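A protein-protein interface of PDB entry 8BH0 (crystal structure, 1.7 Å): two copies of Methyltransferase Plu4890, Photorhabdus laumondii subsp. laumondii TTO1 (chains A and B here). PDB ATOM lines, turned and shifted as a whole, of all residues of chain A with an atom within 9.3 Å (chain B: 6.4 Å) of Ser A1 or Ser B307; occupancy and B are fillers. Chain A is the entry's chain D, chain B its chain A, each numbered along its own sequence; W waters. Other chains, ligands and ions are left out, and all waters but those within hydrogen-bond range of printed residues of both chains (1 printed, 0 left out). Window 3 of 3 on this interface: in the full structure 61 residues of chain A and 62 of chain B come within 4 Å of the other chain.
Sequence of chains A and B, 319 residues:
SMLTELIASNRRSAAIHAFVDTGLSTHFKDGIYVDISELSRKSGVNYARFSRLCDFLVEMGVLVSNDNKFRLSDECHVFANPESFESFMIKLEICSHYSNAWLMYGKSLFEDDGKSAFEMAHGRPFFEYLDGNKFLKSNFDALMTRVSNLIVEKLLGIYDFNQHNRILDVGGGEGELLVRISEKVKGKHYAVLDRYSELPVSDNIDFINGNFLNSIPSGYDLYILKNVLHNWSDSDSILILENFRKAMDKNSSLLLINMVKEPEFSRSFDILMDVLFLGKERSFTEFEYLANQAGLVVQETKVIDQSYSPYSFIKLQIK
Of the 10 printed residues of chain B, 4 touch a printed residue of chain A.
Hydrophobic or aromatic side chains of chain A that line the printed part of chain B: Leu A3.
Among the printed residues, 5 pairs touch across the chains.
Ser A1 touches Ser B307 (CB to O, 3.2 Å).
Glu B75 touches Leu A3 (O to CD2, 3.5 Å).
CZ of Phe B85 touches CG2 of Thr A4, at 3.7 Å.
Thr A4 touches Tyr B308.
Water W1 lies within hydrogen-bond range of OG of Ser B307 (2.7 Å) and OG of Ser A1 (2.9 Å).
The side-chain hydroxyl of Thr A4 sits at hydrogen-bond distance from the side-chain hydroxyl of Ser A1, at 2.7 Å.
Ser A1 touches just these residues of chain B: Ser B307 and Tyr B308.
Met A2 touches none of the printed residues of chain B.
Printed residues of chain B within 4 Å of Leu A3: Glu B75 (3.5 Å).
Of the printed residues of chain B, Thr A4 touches Phe B85 and Tyr B308.
Printed residues of chain A within 4 Å of Glu B75: Leu A3 (3.5 Å).
Of the printed residues of chain A, Phe B85 touches Thr A4 (3.7 Å).
No residue of chain A comes within 4 Å of Gln B306.
Ser B307 touches just one residue of chain A: Ser A1 (3.2 Å).
Printed residues of chain A within 4 Å of Tyr B308: Ser A1 (3.1 Å) and Thr A4 (3.7 Å).
The nearest residue of chain A that does not touch Ser B307 is Met A2 (5.8 Å).
The nearest printed residue of chain A that does not touch Phe B85 is Ser A1 (6.1 Å).
No position is printed for both chains.
Of the 5 pairs that touch across the chains among the printed residues, none has its exchanged pair printed and touching as well.
O of Tyr B308 lies within hydrogen-bond range of N of Ser A1 (3.1 Å).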
ATOM      1  N   SER A   1       8.848 -22.701 -11.034  1.00  0.00           N
ATOM      2  CA  SER A   1       9.268 -24.128 -11.135  1.00  0.00           C
ATOM      3  C   SER A   1      10.657 -24.300 -10.519  1.00  0.00           C
ATOM      4  O   SER A   1      11.367 -23.286 -10.356  1.00  0.00           O
ATOM      5  CB  SER A   1       9.261 -24.613 -12.563  1.00  0.00           C
ATOM      6  OG  SER A   1      10.202 -23.898 -13.354  1.00  0.00           O
ATOM      7  N   MET A   2      11.032 -25.542 -10.212  1.00  0.00           N
ATOM      8  CA  MET A   2      12.389 -25.889  -9.723  1.00  0.00           C
ATOM      9  C   MET A   2      13.399 -25.704 -10.863  1.00  0.00           C
ATOM     10  O   MET A   2      14.515 -25.242 -10.566  1.00  0.00           O
ATOM     11  CB  MET A   2      12.444 -27.324  -9.192  1.00  0.00           C
ATOM     12  CG  MET A   2      11.683 -27.519  -7.886  1.00  0.00           C
ATOM     13  SD  MET A   2      12.378 -26.580  -6.495  1.00  0.00           S
ATOM     14  CE  MET A   2      11.314 -25.138  -6.486  1.00  0.00           C
ATOM     15  N   LEU A   3      13.024 -26.006 -12.116  1.00  0.00           N
ATOM     16  CA  LEU A   3      13.964 -25.953 -13.273  1.00  0.00           C
ATOM     17  C   LEU A   3      14.346 -24.501 -13.579  1.00  0.00           C
ATOM     18  O   LEU A   3      15.550 -24.246 -13.739  1.00  0.00           O
ATOM     19  CB  LEU A   3      13.367 -26.624 -14.514  1.00  0.00           C
ATOM     20  CG  LEU A   3      14.298 -26.656 -15.727  1.00  0.00           C
ATOM     21  CD1 LEU A   3      15.659 -27.236 -15.358  1.00  0.00           C
ATOM     22  CD2 LEU A   3      13.683 -27.437 -16.877  1.00  0.00           C
ATOM     23  N   THR A   4      13.377 -23.585 -13.681  1.00  0.00           N
ATOM     24  CA  THR A   4      13.647 -22.158 -14.012  1.00  0.00           C
ATOM     25  C   THR A   4      14.490 -21.532 -12.892  1.00  0.00           C
ATOM     26  O   THR A   4      15.360 -20.705 -13.213  1.00  0.00           O
ATOM     27  CB  THR A   4      12.362 -21.370 -14.290  1.00  0.00           C
ATOM     28  OG1 THR A   4      11.470 -21.533 -13.187  1.00  0.00           O
ATOM     29  CG2 THR A   4      11.691 -21.803 -15.575  1.00  0.00           C
ATOM     30  N   GLU A   5      14.267 -21.928 -11.636  1.00  0.00           N
ATOM     31  CA  GLU A   5      15.056 -21.423 -10.480  1.00  0.00           C
ATOM     32  C   GLU A   5      16.463 -22.036 -10.512  1.00  0.00           C
ATOM     33  O   GLU A   5      17.408 -21.332 -10.112  1.00  0.00           O
ATOM     34  CB  GLU A   5      14.327 -21.675  -9.159  1.00  0.00           C
ATOM     35  CG  GLU A   5      13.087 -20.810  -8.988  1.00  0.00           C
ATOM     36  CD  GLU A   5      13.302 -19.319  -9.201  1.00  0.00           C
ATOM     37  OE1 GLU A   5      14.382 -18.813  -8.822  1.00  0.00           O
ATOM     38  OE2 GLU A   5      12.390 -18.666  -9.750  1.00  0.00           O
ATOM     39  N   LEU A   6      16.611 -23.275 -10.995  1.00  0.00           N
ATOM     40  CA  LEU A   6      17.943 -23.912 -11.191  1.00  0.00           C
ATOM     41  C   LEU A   6      18.696 -23.163 -12.297  1.00  0.00           C
ATOM     42  O   LEU A   6      19.887 -22.867 -12.103  1.00  0.00           O
ATOM     43  CB  LEU A   6      17.783 -25.395 -11.538  1.00  0.00           C
ATOM     44  CG  LEU A   6      19.092 -26.159 -11.737  1.00  0.00           C
ATOM     45  CD1 LEU A   6      19.910 -26.187 -10.454  1.00  0.00           C
ATOM     46  CD2 LEU A   6      18.829 -27.573 -12.234  1.00  0.00           C
ATOM     47  N   ILE A   7      18.022 -22.865 -13.413  1.00  0.00           N
ATOM     48  CA  ILE A   7      18.594 -22.049 -14.526  1.00  0.00           C
ATOM     49  C   ILE A   7      19.054 -20.701 -13.950  1.00  0.00           C
ATOM     50  O   ILE A   7      20.135 -20.228 -14.353  1.00  0.00           O
ATOM     51  CB  ILE A   7      17.582 -21.890 -15.683  1.00  0.00           C
ATOM     52  CG1 ILE A   7      17.340 -23.221 -16.399  1.00  0.00           C
ATOM     53  CG2 ILE A   7      18.025 -20.805 -16.654  1.00  0.00           C
ATOM     54  CD1 ILE A   7      16.156 -23.211 -17.342  1.00  0.00           C
ATOM     55  N   ALA A   8      18.282 -20.142 -13.010  1.00  0.00           N
ATOM     56  CA  ALA A   8      18.484 -18.801 -12.407  1.00  0.00           C
ATOM     57  C   ALA A   8      19.337 -18.887 -11.131  1.00  0.00           C
ATOM     58  O   ALA A   8      19.278 -17.938 -10.327  1.00  0.00           O
ATOM     59  CB  ALA A   8      17.141 -18.172 -12.124  1.00  0.00           C
ATOM     60  N   ARG A  11      21.444 -15.873  -9.868  1.00  0.00           N
ATOM     61  CA  ARG A  11      20.794 -14.742  -9.149  1.00  0.00           C
ATOM     62  C   ARG A  11      21.131 -14.809  -7.654  1.00  0.00           C
ATOM     63  O   ARG A  11      21.196 -13.741  -7.026  1.00  0.00           O
ATOM     64  CB  ARG A  11      19.280 -14.749  -9.373  1.00  0.00           C
ATOM     65  CG  ARG A  11      18.893 -14.623 -10.836  1.00  0.00           C
ATOM     66  CD  ARG A  11      17.399 -14.560 -11.048  1.00  0.00           C
ATOM     67  NE  ARG A  11      17.073 -14.832 -12.438  1.00  0.00           N
ATOM     68  CZ  ARG A  11      15.860 -15.136 -12.888  1.00  0.00           C
ATOM     69  NH1 ARG A  11      15.682 -15.383 -14.175  1.00  0.00           N
ATOM     70  NH2 ARG A  11      14.834 -15.201 -12.054  1.00  0.00           N
ATOM     71  N   ARG A  12      21.341 -16.013  -7.111  1.00  0.00           N
ATOM     72  CA  ARG A  12      21.696 -16.218  -5.680  1.00  0.00           C
ATOM     73  C   ARG A  12      23.100 -15.649  -5.434  1.00  0.00           C
ATOM     74  O   ARG A  12      23.266 -14.897  -4.455  1.00  0.00           O
ATOM     75  CB  ARG A  12      21.614 -17.698  -5.294  1.00  0.00           C
ATOM     76  CG  ARG A  12      20.200 -18.206  -5.046  1.00  0.00           C
ATOM     77  CD  ARG A  12      19.395 -18.447  -6.308  1.00  0.00           C
ATOM     78  NE  ARG A  12      18.022 -18.825  -5.997  1.00  0.00           N
ATOM     79  CZ  ARG A  12      17.016 -18.835  -6.869  1.00  0.00           C
ATOM     80  NH1 ARG A  12      15.807 -19.196  -6.469  1.00  0.00           N
ATOM     81  NH2 ARG A  12      17.211 -18.486  -8.130  1.00  0.00           N
ATOM     82  N   GLU A  59      14.979 -15.893   1.966  1.00  0.00           N
ATOM     83  CA  GLU A  59      14.607 -17.104   1.182  1.00  0.00           C
ATOM     84  C   GLU A  59      15.824 -18.030   1.032  1.00  0.00           C
ATOM     85  O   GLU A  59      15.663 -19.260   1.159  1.00  0.00           O
ATOM     86  CB  GLU A  59      14.050 -16.673  -0.176  1.00  0.00           C
ATOM     87  CG  GLU A  59      13.673 -17.819  -1.094  1.00  0.00           C
ATOM     88  CD  GLU A  59      13.357 -17.356  -2.504  1.00  0.00           C
ATOM     89  OE1 GLU A  59      13.863 -17.980  -3.461  1.00  0.00           O
ATOM     90  OE2 GLU A  59      12.623 -16.358  -2.637  1.00  0.00           O
ATOM     91  N   GLU B  75      11.803 -33.617 -16.507  1.00  0.00           N
ATOM     92  CA  GLU B  75      11.580 -32.150 -16.375  1.00  0.00           C
ATOM     93  C   GLU B  75      12.459 -31.395 -17.385  1.00  0.00           C
ATOM     94  O   GLU B  75      11.998 -30.357 -17.904  1.00  0.00           O
ATOM     95  CB  GLU B  75      11.882 -31.697 -14.945  1.00  0.00           C
ATOM     96  CG  GLU B  75      11.088 -30.480 -14.509  1.00  0.00           C
ATOM     97  CD  GLU B  75      11.309 -30.078 -13.061  1.00  0.00           C
ATOM     98  OE1 GLU B  75      10.316 -29.997 -12.311  1.00  0.00           O
ATOM     99  OE2 GLU B  75      12.475 -29.846 -12.686  1.00  0.00           O
ATOM    100  N   PHE B  85      11.577 -22.307 -24.508  1.00  0.00           N
ATOM    101  CA  PHE B  85      11.753 -21.018 -23.788  1.00  0.00           C
ATOM    102  C   PHE B  85      12.962 -21.150 -22.851  1.00  0.00           C
ATOM    103  O   PHE B  85      13.723 -20.173 -22.720  1.00  0.00           O
ATOM    104  CB  PHE B  85      10.457 -20.585 -23.090  1.00  0.00           C
ATOM    105  CG  PHE B  85      10.361 -20.880 -21.614  1.00  0.00           C
ATOM    106  CD1 PHE B  85      11.055 -20.112 -20.691  1.00  0.00           C
ATOM    107  CD2 PHE B  85       9.545 -21.897 -21.143  1.00  0.00           C
ATOM    108  CE1 PHE B  85      10.959 -20.375 -19.332  1.00  0.00           C
ATOM    109  CE2 PHE B  85       9.447 -22.157 -19.786  1.00  0.00           C
ATOM    110  CZ  PHE B  85      10.153 -21.396 -18.883  1.00  0.00           C
ATOM    111  N   GLU B  86      13.159 -22.336 -22.262  1.00  0.00           N
ATOM    112  CA  GLU B  86      14.268 -22.626 -21.312  1.00  0.00           C
ATOM    113  C   GLU B  86      15.617 -22.443 -22.019  1.00  0.00           C
ATOM    114  O   GLU B  86      16.555 -21.942 -21.369  1.00  0.00           O
ATOM    115  CB  GLU B  86      14.145 -24.033 -20.723  1.00  0.00           C
ATOM    116  CG  GLU B  86      12.957 -24.206 -19.788  1.00  0.00           C
ATOM    117  CD  GLU B  86      11.657 -24.640 -20.449  1.00  0.00           C
ATOM    118  OE1 GLU B  86      11.567 -24.572 -21.693  1.00  0.00           O
ATOM    119  OE2 GLU B  86      10.737 -25.053 -19.716  1.00  0.00           O
ATOM    120  N   LEU B 150       2.957 -20.926 -24.804  1.00  0.00           N
ATOM    121  CA  LEU B 150       2.640 -21.934 -23.753  1.00  0.00           C
ATOM    122  C   LEU B 150       1.314 -21.600 -23.054  1.00  0.00           C
ATOM    123  O   LEU B 150       0.677 -22.548 -22.556  1.00  0.00           O
ATOM    124  CB  LEU B 150       3.786 -21.998 -22.738  1.00  0.00           C
ATOM    125  CG  LEU B 150       5.100 -22.575 -23.264  1.00  0.00           C
ATOM    126  CD1 LEU B 150       6.226 -22.352 -22.266  1.00  0.00           C
ATOM    127  CD2 LEU B 150       4.960 -24.054 -23.588  1.00  0.00           C
ATOM    128  N   PHE B 265       6.503 -18.940  -3.888  1.00  0.00           N
ATOM    129  CA  PHE B 265       7.419 -18.948  -5.060  1.00  0.00           C
ATOM    130  C   PHE B 265       8.629 -18.048  -4.778  1.00  0.00           C
ATOM    131  O   PHE B 265       8.567 -17.196  -3.872  1.00  0.00           O
ATOM    132  CB  PHE B 265       6.658 -18.545  -6.326  1.00  0.00           C
ATOM    133  CG  PHE B 265       5.649 -19.571  -6.777  1.00  0.00           C
ATOM    134  CD1 PHE B 265       5.987 -20.535  -7.714  1.00  0.00           C
ATOM    135  CD2 PHE B 265       4.367 -19.590  -6.246  1.00  0.00           C
ATOM    136  CE1 PHE B 265       5.063 -21.484  -8.123  1.00  0.00           C
ATOM    137  CE2 PHE B 265       3.444 -20.540  -6.654  1.00  0.00           C
ATOM    138  CZ  PHE B 265       3.794 -21.487  -7.590  1.00  0.00           C
ATOM    139  N   ASP B 305      -2.404 -21.280 -14.043  1.00  0.00           N
ATOM    140  CA  ASP B 305      -1.184 -22.047 -13.684  1.00  0.00           C
ATOM    141  C   ASP B 305      -0.298 -22.153 -14.928  1.00  0.00           C
ATOM    142  O   ASP B 305      -0.808 -22.574 -15.982  1.00  0.00           O
ATOM    143  CB  ASP B 305      -1.530 -23.434 -13.137  1.00  0.00           C
ATOM    144  CG  ASP B 305      -2.321 -23.415 -11.840  1.00  0.00           C
ATOM    145  OD1 ASP B 305      -2.240 -22.404 -11.112  1.00  0.00           O
ATOM    146  OD2 ASP B 305      -3.015 -24.415 -11.567  1.00  0.00           O
ATOM    147  N   GLN B 306       0.967 -21.747 -14.808  1.00  0.00           N
ATOM    148  CA  GLN B 306       2.055 -22.100 -15.757  1.00  0.00           C
ATOM    149  C   GLN B 306       3.146 -22.808 -14.951  1.00  0.00           C
ATOM    150  O   GLN B 306       3.224 -22.565 -13.729  1.00  0.00           O
ATOM    151  CB  GLN B 306       2.566 -20.858 -16.490  1.00  0.00           C
ATOM    152  CG  GLN B 306       1.549 -20.258 -17.452  1.00  0.00           C
ATOM    153  CD  GLN B 306       1.276 -21.163 -18.630  1.00  0.00           C
ATOM    154  OE1 GLN B 306       0.339 -21.958 -18.623  1.00  0.00           O
ATOM    155  NE2 GLN B 306       2.114 -21.068 -19.649  1.00  0.00           N
ATOM    156  N   SER B 307       3.932 -23.669 -15.602  1.00  0.00           N
ATOM    157  CA  SER B 307       4.942 -24.547 -14.955  1.00  0.00           C
ATOM    158  C   SER B 307       5.852 -23.719 -14.040  1.00  0.00           C
ATOM    159  O   SER B 307       6.139 -24.183 -12.921  1.00  0.00           O
ATOM    160  CB  SER B 307       5.740 -25.307 -15.984  1.00  0.00           C
ATOM    161  OG  SER B 307       6.495 -24.422 -16.798  1.00  0.00           O
ATOM    162  N   TYR B 308       6.239 -22.519 -14.485  1.00  0.00           N
ATOM    163  CA  TYR B 308       7.324 -21.687 -13.896  1.00  0.00           C
ATOM    164  C   TYR B 308       6.765 -20.619 -12.945  1.00  0.00           C
ATOM    165  O   TYR B 308       7.551 -20.092 -12.139  1.00  0.00           O
ATOM    166  CB  TYR B 308       8.153 -21.032 -15.004  1.00  0.00           C
ATOM    167  CG  TYR B 308       7.346 -20.217 -15.981  1.00  0.00           C
ATOM    168  CD1 TYR B 308       7.004 -18.904 -15.706  1.00  0.00           C
ATOM    169  CD2 TYR B 308       6.902 -20.769 -17.172  1.00  0.00           C
ATOM    170  CE1 TYR B 308       6.243 -18.157 -16.590  1.00  0.00           C
ATOM    171  CE2 TYR B 308       6.145 -20.034 -18.070  1.00  0.00           C
ATOM    172  CZ  TYR B 308       5.816 -18.723 -17.779  1.00  0.00           C
ATOM    173  OH  TYR B 308       5.075 -17.988 -18.655  1.00  0.00           O
ATOM    174  N   SER B 309       5.474 -20.282 -13.039  1.00  0.00           N
ATOM    175  CA  SER B 309       4.859 -19.176 -12.258  1.00  0.00           C
ATOM    176  C   SER B 309       3.336 -19.246 -12.312  1.00  0.00           C
ATOM    177  O   SER B 309       2.767 -19.659 -13.320  1.00  0.00           O
ATOM    178  CB  SER B 309       5.340 -17.838 -12.761  1.00  0.00           C
ATOM    179  OG  SER B 309       4.737 -16.774 -12.038  1.00  0.00           O
HETATM  180  O   HOH W   1       9.044 -24.539 -15.966  1.00  0.00           O
